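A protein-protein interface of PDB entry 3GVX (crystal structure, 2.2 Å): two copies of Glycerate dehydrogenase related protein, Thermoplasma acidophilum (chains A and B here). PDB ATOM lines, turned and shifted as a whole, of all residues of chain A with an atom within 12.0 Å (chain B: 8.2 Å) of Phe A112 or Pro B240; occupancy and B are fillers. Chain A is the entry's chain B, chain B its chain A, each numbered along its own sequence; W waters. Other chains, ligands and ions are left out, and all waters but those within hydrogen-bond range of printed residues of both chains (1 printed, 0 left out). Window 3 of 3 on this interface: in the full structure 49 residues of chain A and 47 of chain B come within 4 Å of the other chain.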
ATOM      1  N   ASN A  99       6.641  27.369  36.337  1.00  0.00           N
ATOM      2  CA  ASN A  99       6.141  26.045  35.984  1.00  0.00           C
ATOM      3  C   ASN A  99       6.961  25.492  34.836  1.00  0.00           C
ATOM      4  O   ASN A  99       6.430  24.980  33.858  1.00  0.00           O
ATOM      5  CB  ASN A  99       4.666  26.132  35.585  1.00  0.00           C
ATOM      6  CG  ASN A  99       3.794  26.635  36.714  1.00  0.00           C
ATOM      7  OD1 ASN A  99       2.864  27.419  36.494  1.00  0.00           O
ATOM      8  ND2 ASN A  99       4.078  26.182  37.933  1.00  0.00           N
ATOM      9  N   GLU A 102       6.594  21.318  34.157  1.00  0.00           N
ATOM     10  CA  GLU A 102       5.288  20.956  33.650  1.00  0.00           C
ATOM     11  C   GLU A 102       5.036  21.472  32.234  1.00  0.00           C
ATOM     12  O   GLU A 102       4.572  20.732  31.376  1.00  0.00           O
ATOM     13  CB  GLU A 102       4.212  21.451  34.620  1.00  0.00           C
ATOM     14  CG  GLU A 102       4.482  21.033  36.070  1.00  0.00           C
ATOM     15  CD  GLU A 102       5.311  22.051  36.853  1.00  0.00           C
ATOM     16  OE1 GLU A 102       6.161  22.738  36.252  1.00  0.00           O
ATOM     17  OE2 GLU A 102       5.102  22.152  38.078  1.00  0.00           O
ATOM     18  N   ASN A 103       5.344  22.739  31.981  1.00  0.00           N
ATOM     19  CA  ASN A 103       5.154  23.293  30.645  1.00  0.00           C
ATOM     20  C   ASN A 103       6.058  22.623  29.620  1.00  0.00           C
ATOM     21  O   ASN A 103       5.643  22.343  28.511  1.00  0.00           O
ATOM     22  CB  ASN A 103       5.413  24.803  30.619  1.00  0.00           C
ATOM     23  CG  ASN A 103       4.362  25.588  31.352  1.00  0.00           C
ATOM     24  OD1 ASN A 103       3.222  25.150  31.472  1.00  0.00           O
ATOM     25  ND2 ASN A 103       4.732  26.771  31.833  1.00  0.00           N
ATOM     26  N   ASN A 104       7.297  22.362  30.011  1.00  0.00           N
ATOM     27  CA  ASN A 104       8.235  21.741  29.102  1.00  0.00           C
ATOM     28  C   ASN A 104       7.770  20.350  28.727  1.00  0.00           C
ATOM     29  O   ASN A 104       7.864  19.952  27.568  1.00  0.00           O
ATOM     30  CB  ASN A 104       9.630  21.699  29.707  1.00  0.00           C
ATOM     31  CG  ASN A 104      10.603  20.926  28.857  1.00  0.00           C
ATOM     32  OD1 ASN A 104      11.010  19.816  29.216  1.00  0.00           O
ATOM     33  ND2 ASN A 104      10.988  21.504  27.721  1.00  0.00           N
ATOM     34  N   GLU A 105       7.276  19.612  29.711  1.00  0.00           N
ATOM     35  CA  GLU A 105       6.757  18.281  29.447  1.00  0.00           C
ATOM     36  C   GLU A 105       5.637  18.351  28.424  1.00  0.00           C
ATOM     37  O   GLU A 105       5.599  17.577  27.488  1.00  0.00           O
ATOM     38  CB  GLU A 105       6.240  17.634  30.721  1.00  0.00           C
ATOM     39  CG  GLU A 105       5.586  16.306  30.479  1.00  0.00           C
ATOM     40  CD  GLU A 105       5.072  15.701  31.770  1.00  0.00           C
ATOM     41  OE1 GLU A 105       4.059  16.187  32.323  1.00  0.00           O
ATOM     42  OE2 GLU A 105       5.699  14.741  32.246  1.00  0.00           O
ATOM     43  N   LEU A 106       4.716  19.283  28.613  1.00  0.00           N
ATOM     44  CA  LEU A 106       3.608  19.460  27.683  1.00  0.00           C
ATOM     45  C   LEU A 106       4.076  19.879  26.297  1.00  0.00           C
ATOM     46  O   LEU A 106       3.718  19.254  25.318  1.00  0.00           O
ATOM     47  CB  LEU A 106       2.573  20.451  28.263  1.00  0.00           C
ATOM     48  CG  LEU A 106       1.304  19.892  28.927  1.00  0.00           C
ATOM     49  CD1 LEU A 106       1.595  18.584  29.606  1.00  0.00           C
ATOM     50  CD2 LEU A 106       0.725  20.948  29.843  1.00  0.00           C
ATOM     51  N   MET A 107       4.870  20.937  26.209  1.00  0.00           N
ATOM     52  CA  MET A 107       5.375  21.408  24.915  1.00  0.00           C
ATOM     53  C   MET A 107       6.082  20.325  24.092  1.00  0.00           C
ATOM     54  O   MET A 107       5.923  20.241  22.883  1.00  0.00           O
ATOM     55  CB  MET A 107       6.332  22.596  25.103  1.00  0.00           C
ATOM     56  CG  MET A 107       5.674  23.874  25.561  1.00  0.00           C
ATOM     57  SD  MET A 107       4.692  24.648  24.259  1.00  0.00           S
ATOM     58  CE  MET A 107       5.836  24.889  23.064  1.00  0.00           C
ATOM     59  N   LYS A 108       6.865  19.487  24.750  1.00  0.00           N
ATOM     60  CA  LYS A 108       7.585  18.446  24.033  1.00  0.00           C
ATOM     61  C   LYS A 108       6.750  17.327  23.446  1.00  0.00           C
ATOM     62  O   LYS A 108       7.204  16.606  22.566  1.00  0.00           O
ATOM     63  CB  LYS A 108       8.683  17.873  24.909  1.00  0.00           C
ATOM     64  CG  LYS A 108       9.918  18.668  24.754  1.00  0.00           C
ATOM     65  CD  LYS A 108      10.952  18.369  25.778  1.00  0.00           C
ATOM     66  CE  LYS A 108      12.240  19.018  25.344  1.00  0.00           C
ATOM     67  NZ  LYS A 108      13.378  18.627  26.200  1.00  0.00           N
ATOM     68  N   ALA A 109       5.534  17.185  23.947  1.00  0.00           N
ATOM     69  CA  ALA A 109       4.626  16.183  23.434  1.00  0.00           C
ATOM     70  C   ALA A 109       3.697  16.859  22.420  1.00  0.00           C
ATOM     71  O   ALA A 109       2.704  16.288  22.000  1.00  0.00           O
ATOM     72  CB  ALA A 109       3.833  15.566  24.582  1.00  0.00           C
ATOM     73  N   GLY A 110       4.036  18.090  22.035  1.00  0.00           N
ATOM     74  CA  GLY A 110       3.238  18.835  21.074  1.00  0.00           C
ATOM     75  C   GLY A 110       1.955  19.432  21.622  1.00  0.00           C
ATOM     76  O   GLY A 110       1.057  19.787  20.863  1.00  0.00           O
ATOM     77  N   ILE A 111       1.861  19.545  22.942  1.00  0.00           N
ATOM     78  CA  ILE A 111       0.672  20.110  23.567  1.00  0.00           C
ATOM     79  C   ILE A 111       0.975  21.533  23.993  1.00  0.00           C
ATOM     80  O   ILE A 111       1.788  21.781  24.891  1.00  0.00           O
ATOM     81  CB  ILE A 111       0.224  19.283  24.794  1.00  0.00           C
ATOM     82  CG1 ILE A 111      -0.058  17.845  24.346  1.00  0.00           C
ATOM     83  CG2 ILE A 111      -1.009  19.920  25.442  1.00  0.00           C
ATOM     84  CD1 ILE A 111      -0.109  16.850  25.458  1.00  0.00           C
ATOM     85  N   PHE A 112       0.330  22.470  23.308  1.00  0.00           N
ATOM     86  CA  PHE A 112       0.521  23.884  23.577  1.00  0.00           C
ATOM     87  C   PHE A 112      -0.541  24.321  24.535  1.00  0.00           C
ATOM     88  O   PHE A 112      -1.713  24.409  24.196  1.00  0.00           O
ATOM     89  CB  PHE A 112       0.393  24.722  22.321  1.00  0.00           C
ATOM     90  CG  PHE A 112       0.743  26.168  22.527  1.00  0.00           C
ATOM     91  CD1 PHE A 112       2.060  26.576  22.520  1.00  0.00           C
ATOM     92  CD2 PHE A 112      -0.239  27.121  22.697  1.00  0.00           C
ATOM     93  CE1 PHE A 112       2.394  27.912  22.673  1.00  0.00           C
ATOM     94  CE2 PHE A 112       0.094  28.468  22.853  1.00  0.00           C
ATOM     95  CZ  PHE A 112       1.412  28.857  22.839  1.00  0.00           C
ATOM     96  N   ARG A 113      -0.138  24.637  25.744  1.00  0.00           N
ATOM     97  CA  ARG A 113      -1.143  25.007  26.681  1.00  0.00           C
ATOM     98  C   ARG A 113      -0.719  26.031  27.697  1.00  0.00           C
ATOM     99  O   ARG A 113       0.065  25.764  28.599  1.00  0.00           O
ATOM    100  CB  ARG A 113      -1.605  23.756  27.346  1.00  0.00           C
ATOM    101  CG  ARG A 113      -2.625  23.977  28.332  1.00  0.00           C
ATOM    102  CD  ARG A 113      -2.387  22.930  29.323  1.00  0.00           C
ATOM    103  NE  ARG A 113      -3.643  22.563  29.930  1.00  0.00           N
ATOM    104  CZ  ARG A 113      -4.001  22.933  31.145  1.00  0.00           C
ATOM    105  NH1 ARG A 113      -3.181  23.671  31.873  1.00  0.00           N
ATOM    106  NH2 ARG A 113      -5.180  22.585  31.616  1.00  0.00           N
ATOM    107  N   GLN A 114      -1.292  27.209  27.548  1.00  0.00           N
ATOM    108  CA  GLN A 114      -0.947  28.309  28.401  1.00  0.00           C
ATOM    109  C   GLN A 114      -1.557  28.272  29.765  1.00  0.00           C
ATOM    110  O   GLN A 114      -2.673  27.812  29.974  1.00  0.00           O
ATOM    111  CB  GLN A 114      -1.291  29.619  27.718  1.00  0.00           C
ATOM    112  CG  GLN A 114      -0.666  29.739  26.375  1.00  0.00           C
ATOM    113  CD  GLN A 114      -0.721  31.143  25.873  1.00  0.00           C
ATOM    114  OE1 GLN A 114      -1.758  31.798  25.951  1.00  0.00           O
ATOM    115  NE2 GLN A 114       0.398  31.629  25.354  1.00  0.00           N
ATOM    116  N   SER A 115      -0.779  28.786  30.694  1.00  0.00           N
ATOM    117  CA  SER A 115      -1.186  28.861  32.064  1.00  0.00           C
ATOM    118  C   SER A 115      -0.354  29.961  32.701  1.00  0.00           C
ATOM    119  O   SER A 115       0.757  30.243  32.274  1.00  0.00           O
ATOM    120  CB  SER A 115      -0.935  27.527  32.752  1.00  0.00           C
ATOM    121  OG  SER A 115      -1.460  27.551  34.052  1.00  0.00           O
ATOM    122  N   PRO A 116      -0.906  30.612  33.716  1.00  0.00           N
ATOM    123  CA  PRO A 116      -0.186  31.684  34.390  1.00  0.00           C
ATOM    124  C   PRO A 116       0.986  31.221  35.237  1.00  0.00           C
ATOM    125  O   PRO A 116       1.049  30.072  35.682  1.00  0.00           O
ATOM    126  CB  PRO A 116      -1.278  32.379  35.211  1.00  0.00           C
ATOM    127  CG  PRO A 116      -2.288  31.288  35.429  1.00  0.00           C
ATOM    128  CD  PRO A 116      -2.328  30.618  34.086  1.00  0.00           C
ATOM    129  N   ASP B 234      10.515  30.321  24.554  1.00  0.00           N
ATOM    130  CA  ASP B 234       9.165  30.587  24.992  1.00  0.00           C
ATOM    131  C   ASP B 234       8.300  30.727  23.749  1.00  0.00           C
ATOM    132  O   ASP B 234       7.087  30.888  23.835  1.00  0.00           O
ATOM    133  CB  ASP B 234       9.094  31.874  25.818  1.00  0.00           C
ATOM    134  CG  ASP B 234       7.736  32.068  26.471  1.00  0.00           C
ATOM    135  OD1 ASP B 234       7.273  31.136  27.167  1.00  0.00           O
ATOM    136  OD2 ASP B 234       7.134  33.147  26.296  1.00  0.00           O
ATOM    137  N   VAL B 235       8.940  30.673  22.588  1.00  0.00           N
ATOM    138  CA  VAL B 235       8.218  30.780  21.341  1.00  0.00           C
ATOM    139  C   VAL B 235       8.563  29.696  20.345  1.00  0.00           C
ATOM    140  O   VAL B 235       9.693  29.224  20.260  1.00  0.00           O
ATOM    141  CB  VAL B 235       8.429  32.149  20.684  1.00  0.00           C
ATOM    142  CG1 VAL B 235       7.933  33.250  21.613  1.00  0.00           C
ATOM    143  CG2 VAL B 235       9.888  32.325  20.294  1.00  0.00           C
ATOM    144  N   TRP B 236       7.553  29.298  19.592  1.00  0.00           N
ATOM    145  CA  TRP B 236       7.720  28.249  18.623  1.00  0.00           C
ATOM    146  C   TRP B 236       6.982  28.573  17.338  1.00  0.00           C
ATOM    147  O   TRP B 236       6.027  29.341  17.338  1.00  0.00           O
ATOM    148  CB  TRP B 236       7.238  26.935  19.239  1.00  0.00           C
ATOM    149  CG  TRP B 236       7.714  25.746  18.510  1.00  0.00           C
ATOM    150  CD1 TRP B 236       7.065  25.097  17.506  1.00  0.00           C
ATOM    151  CD2 TRP B 236       8.971  25.071  18.677  1.00  0.00           C
ATOM    152  NE1 TRP B 236       7.827  24.072  17.039  1.00  0.00           N
ATOM    153  CE2 TRP B 236       9.004  24.030  17.732  1.00  0.00           C
ATOM    154  CE3 TRP B 236      10.075  25.256  19.521  1.00  0.00           C
ATOM    155  CZ2 TRP B 236      10.075  23.161  17.612  1.00  0.00           C
ATOM    156  CZ3 TRP B 236      11.146  24.394  19.404  1.00  0.00           C
ATOM    157  CH2 TRP B 236      11.138  23.355  18.444  1.00  0.00           C
ATOM    158  N   TRP B 237       7.421  27.977  16.238  1.00  0.00           N
ATOM    159  CA  TRP B 237       6.800  28.243  14.953  1.00  0.00           C
ATOM    160  C   TRP B 237       5.401  27.669  14.830  1.00  0.00           C
ATOM    161  O   TRP B 237       5.161  26.479  15.063  1.00  0.00           O
ATOM    162  CB  TRP B 237       7.671  27.698  13.830  1.00  0.00           C
ATOM    163  CG  TRP B 237       9.098  28.118  13.910  1.00  0.00           C
ATOM    164  CD1 TRP B 237       9.678  29.174  13.277  1.00  0.00           C
ATOM    165  CD2 TRP B 237      10.131  27.497  14.685  1.00  0.00           C
ATOM    166  NE1 TRP B 237      10.998  29.258  13.610  1.00  0.00           N
ATOM    167  CE2 TRP B 237      11.303  28.259  14.483  1.00  0.00           C
ATOM    168  CE3 TRP B 237      10.174  26.402  15.553  1.00  0.00           C
ATOM    169  CZ2 TRP B 237      12.513  27.933  15.079  1.00  0.00           C
ATOM    170  CZ3 TRP B 237      11.374  26.079  16.146  1.00  0.00           C
ATOM    171  CH2 TRP B 237      12.530  26.858  15.918  1.00  0.00           C
ATOM    172  N   ASN B 238       4.476  28.538  14.447  1.00  0.00           N
ATOM    173  CA  ASN B 238       3.085  28.172  14.242  1.00  0.00           C
ATOM    174  C   ASN B 238       2.311  27.730  15.461  1.00  0.00           C
ATOM    175  O   ASN B 238       1.625  26.711  15.429  1.00  0.00           O
ATOM    176  CB  ASN B 238       2.980  27.098  13.162  1.00  0.00           C
ATOM    177  CG  ASN B 238       3.296  27.640  11.789  1.00  0.00           C
ATOM    178  OD1 ASN B 238       2.689  28.622  11.335  1.00  0.00           O
ATOM    179  ND2 ASN B 238       4.252  27.016  11.119  1.00  0.00           N
ATOM    180  N   GLU B 239       2.397  28.512  16.528  1.00  0.00           N
ATOM    181  CA  GLU B 239       1.669  28.183  17.730  1.00  0.00           C
ATOM    182  C   GLU B 239       0.216  28.391  17.329  1.00  0.00           C
ATOM    183  O   GLU B 239      -0.088  29.308  16.576  1.00  0.00           O
ATOM    184  CB  GLU B 239       2.053  29.120  18.867  1.00  0.00           C
ATOM    185  CG  GLU B 239       3.514  29.136  19.158  1.00  0.00           C
ATOM    186  CD  GLU B 239       3.911  30.322  20.016  1.00  0.00           C
ATOM    187  OE1 GLU B 239       5.050  30.338  20.513  1.00  0.00           O
ATOM    188  OE2 GLU B 239       3.087  31.238  20.200  1.00  0.00           O
ATOM    189  N   PRO B 240      -0.700  27.553  17.805  1.00  0.00           N
ATOM    190  CA  PRO B 240      -0.475  26.417  18.687  1.00  0.00           C
ATOM    191  C   PRO B 240      -0.166  25.058  18.047  1.00  0.00           C
ATOM    192  O   PRO B 240       0.140  24.116  18.772  1.00  0.00           O
ATOM    193  CB  PRO B 240      -1.741  26.395  19.531  1.00  0.00           C
ATOM    194  CG  PRO B 240      -2.760  26.754  18.561  1.00  0.00           C
ATOM    195  CD  PRO B 240      -2.119  27.945  17.866  1.00  0.00           C
ATOM    196  N   GLU B 241      -0.207  24.943  16.714  1.00  0.00           N
ATOM    197  CA  GLU B 241       0.124  23.656  16.083  1.00  0.00           C
ATOM    198  C   GLU B 241       1.601  23.518  15.952  1.00  0.00           C
ATOM    199  O   GLU B 241       2.167  23.560  14.855  1.00  0.00           O
ATOM    200  CB  GLU B 241      -0.449  23.491  14.688  1.00  0.00           C
ATOM    201  CG  GLU B 241      -1.118  24.683  14.118  1.00  0.00           C
ATOM    202  CD  GLU B 241      -2.515  24.804  14.641  1.00  0.00           C
ATOM    203  OE1 GLU B 241      -3.099  23.742  14.957  1.00  0.00           O
ATOM    204  OE2 GLU B 241      -3.025  25.942  14.735  1.00  0.00           O
ATOM    205  N   ILE B 242       2.227  23.327  17.088  1.00  0.00           N
ATOM    206  CA  ILE B 242       3.648  23.195  17.121  1.00  0.00           C
ATOM    207  C   ILE B 242       4.030  21.771  16.746  1.00  0.00           C
ATOM    208  O   ILE B 242       3.364  20.807  17.133  1.00  0.00           O
ATOM    209  CB  ILE B 242       4.132  23.544  18.512  1.00  0.00           C
ATOM    210  CG1 ILE B 242       3.386  22.675  19.523  1.00  0.00           C
ATOM    211  CG2 ILE B 242       3.828  25.007  18.797  1.00  0.00           C
ATOM    212  CD1 ILE B 242       3.897  22.761  20.913  1.00  0.00           C
ATOM    213  N   THR B 243       5.098  21.650  15.975  1.00  0.00           N
ATOM    214  CA  THR B 243       5.602  20.359  15.572  1.00  0.00           C
ATOM    215  C   THR B 243       7.104  20.349  15.718  1.00  0.00           C
ATOM    216  O   THR B 243       7.755  21.396  15.702  1.00  0.00           O
ATOM    217  CB  THR B 243       5.304  20.034  14.100  1.00  0.00           C
ATOM    218  OG1 THR B 243       5.960  20.992  13.277  1.00  0.00           O
ATOM    219  CG2 THR B 243       3.800  20.038  13.817  1.00  0.00           C
ATOM    220  N   THR B 245       8.814  19.290  18.330  1.00  0.00           N
ATOM    221  CA  THR B 245       9.201  19.802  19.628  1.00  0.00           C
ATOM    222  C   THR B 245       9.930  18.824  20.525  1.00  0.00           C
ATOM    223  O   THR B 245      10.492  19.221  21.542  1.00  0.00           O
ATOM    224  CB  THR B 245       7.981  20.328  20.396  1.00  0.00           C
ATOM    225  OG1 THR B 245       6.973  19.309  20.450  1.00  0.00           O
ATOM    226  CG2 THR B 245       7.431  21.580  19.722  1.00  0.00           C
ATOM    227  N   SER B 253       8.524  26.446  26.680  1.00  0.00           N
ATOM    228  CA  SER B 253       7.394  26.963  27.406  1.00  0.00           C
ATOM    229  C   SER B 253       6.435  27.502  26.343  1.00  0.00           C
ATOM    230  O   SER B 253       6.864  27.963  25.296  1.00  0.00           O
ATOM    231  CB  SER B 253       7.819  28.047  28.404  1.00  0.00           C
ATOM    232  OG  SER B 253       8.464  29.135  27.783  1.00  0.00           O
ATOM    233  N   PRO B 254       5.123  27.447  26.604  1.00  0.00           N
ATOM    234  CA  PRO B 254       4.095  27.916  25.669  1.00  0.00           C
ATOM    235  C   PRO B 254       3.802  29.421  25.624  1.00  0.00           C
ATOM    236  O   PRO B 254       2.700  29.838  25.929  1.00  0.00           O
ATOM    237  CB  PRO B 254       2.869  27.106  26.085  1.00  0.00           C
ATOM    238  CG  PRO B 254       3.036  27.051  27.584  1.00  0.00           C
ATOM    239  CD  PRO B 254       4.509  26.748  27.748  1.00  0.00           C
ATOM    240  N   HIS B 255       4.797  30.222  25.253  1.00  0.00           N
ATOM    241  CA  HIS B 255       4.598  31.663  25.112  1.00  0.00           C
ATOM    242  C   HIS B 255       3.947  32.325  26.332  1.00  0.00           C
ATOM    243  O   HIS B 255       3.025  33.117  26.189  1.00  0.00           O
ATOM    244  CB  HIS B 255       3.727  31.903  23.870  1.00  0.00           C
ATOM    245  CG  HIS B 255       4.013  33.182  23.152  1.00  0.00           C
ATOM    246  ND1 HIS B 255       3.602  33.420  21.859  1.00  0.00           N
ATOM    247  CD2 HIS B 255       4.697  34.282  23.533  1.00  0.00           C
ATOM    248  CE1 HIS B 255       4.031  34.607  21.474  1.00  0.00           C
ATOM    249  NE2 HIS B 255       4.698  35.151  22.470  1.00  0.00           N
ATOM    250  N   VAL B 256       4.430  32.015  27.530  1.00  0.00           N
ATOM    251  CA  VAL B 256       3.861  32.600  28.739  1.00  0.00           C
ATOM    252  C   VAL B 256       4.818  33.532  29.487  1.00  0.00           C
ATOM    253  O   VAL B 256       4.596  33.856  30.659  1.00  0.00           O
ATOM    254  CB  VAL B 256       3.395  31.489  29.698  1.00  0.00           C
ATOM    255  CG1 VAL B 256       2.218  30.713  29.093  1.00  0.00           C
ATOM    256  CG2 VAL B 256       4.572  30.558  30.025  1.00  0.00           C
ATOM    257  N   MET B 260      -0.893  37.105  28.898  1.00  0.00           N
ATOM    258  CA  MET B 260      -1.626  35.963  28.415  1.00  0.00           C
ATOM    259  C   MET B 260      -2.998  36.244  27.902  1.00  0.00           C
ATOM    260  O   MET B 260      -3.790  37.026  28.432  1.00  0.00           O
ATOM    261  CB  MET B 260      -1.733  34.902  29.469  1.00  0.00           C
ATOM    262  CG  MET B 260      -1.681  33.526  28.904  1.00  0.00           C
ATOM    263  SD  MET B 260      -1.449  32.602  30.393  1.00  0.00           S
ATOM    264  CE  MET B 260       0.110  33.517  31.010  1.00  0.00           C
ATOM    265  N   SER B 261      -3.247  35.590  26.801  1.00  0.00           N
ATOM    266  CA  SER B 261      -4.496  35.663  26.134  1.00  0.00           C
ATOM    267  C   SER B 261      -5.617  35.629  27.207  1.00  0.00           C
ATOM    268  O   SER B 261      -6.550  36.425  27.164  1.00  0.00           O
ATOM    269  CB  SER B 261      -4.505  34.468  25.183  1.00  0.00           C
ATOM    270  OG  SER B 261      -3.190  34.325  24.644  1.00  0.00           O
HETATM  271  O   HOH W   1       0.680  34.589  24.278  1.00  0.00           O
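The side-chain carboxylate (OD1) of Asp B234 lies within hydrogen-bond range of the side-chain hydroxyl (OG) of Ser B253 (2.4 Å). ND1 of His B255 sits at hydrogen-bond distance from OE2 of Glu B239, at 2.8 Å. O of Pro A116 lies close to OD1 of Asn A99. O of Asp B234 is in hydrogen-bond range of N of His B255, at 2.8 Å. The side-chain carboxylate (OD1) of Asp B234 sits at hydrogen-bond distance from the backbone NH (N) of Val B256. The backbone NH (N) of Trp B236 lies within hydrogen-bond range of the side-chain carboxylate (OE1) of Glu B239, 2.9 Å away.
Water W1 lies within hydrogen-bond range of the side-chain amide nitrogen (NE2) of Gln A114 (3.2 Å) and the backbone carbonyl oxygen (O) of His B255 (3.4 Å).
The side-chain hydroxyl of Ser B261 sits at hydrogen-bond distance from the side-chain amide oxygen of Gln A114, 3.2 Å away. O of Ser A115 sits close to SD of Met B260 (3.7 Å). The side-chain hydroxyl (OG1) of Thr B245 is in hydrogen-bond range of the backbone carbonyl oxygen (O) of Met A107 (2.8 Å). The backbone carbonyl oxygen of His B255 is in hydrogen-bond range of the side-chain amide nitrogen of Gln A114 (3.1 Å). The side-chain amide nitrogen of Gln A114 sits at hydrogen-bond distance from the backbone carbonyl oxygen of Pro B254 (3.0 Å). The side-chain hydroxyl (OG1) of Thr B245 lies within hydrogen-bond range of the backbone carbonyl oxygen (O) of Lys A108. SD of Met A107 lies close to N of Pro B254.
Among the printed residues, pairs that only touch across the chains: Arg A113 with Pro B254, Gln A114 with Met B260, Phe A112 with Pro B254, Ser A115 with Val B256, Gly A110 with Thr B245, Phe A112 with Pro B240, Asn A103 with Pro B254, Met A107 with Ile B242, Met A107 with Ser B253, Pro A116 with Met B260, Phe A112 with Glu B239, Gly A110 with Ile B242, Gln A114 with Val B256 and Phe A112 with His B255.
Of chain B, only Glu B239, Pro B240, Pro B254 and His B255 come within 4 Å of Phe A112. Of chain A, only Phe A112 comes within 4 Å of Pro B240. No residue of chain A comes within 4 Å of Glu B241. Ile B242 touches just these residues of chain A: Met A107 and Gly A110. Of the printed residues of chain A, Pro B254 touches Asn A103, Met A107, Phe A112, Arg A113 and Gln A114. Of the printed residues of chain B, Gly A110 touches Ile B242 and Thr B245. Printed residues of chain B within 4 Å of Met A107: Ile B242 (3.6 Å), Thr B245 (2.8 Å), Ser B253 (3.8 Å) and Pro B254 (3.6 Å). Of the printed residues of chain B, Asn A103 touches Pro B254. Of the printed residues of chain A, Thr B245 touches Met A107 (2.8 Å), Lys A108 (3.3 Å) and Gly A110 (3.6 Å). Of the printed residues of chain A, Val B256 touches Gln A114 (3.9 Å) and Ser A115 (3.5 Å). Val B235 touches none of the printed residues of chain A. Glu A102 touches none of the printed residues of chain B. The nearest residue of chain B that does not touch Phe A112 is Ile B242 (4.3 Å). The nearest printed residue of chain B that does not touch Ser A115 is Pro B254 (5.2 Å).
No position is printed for both chains.
Printed residues of chain A that touch a printed residue of chain B: Asn A103, Met A107, Lys A108, Gly A110, Phe A112, Arg A113, Gln A114, Ser A115 and Pro A116. Hydrophobic or aromatic side chains of chain A within 4 Å of the printed part of chain B: Met A107 and Phe A112. Hydrophobic or aromatic side chains of chain B within 4 Å of the printed part of chain A: Pro B240, Ile B242, Pro B254, His B255, Val B256 and Met B260. Among the printed residues, 21 pairs touch across the chains. Among the printed residues, no Asp or Glu carboxylate lies within 4 Å of a Lys or Arg side-chain nitrogen of the other chain.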
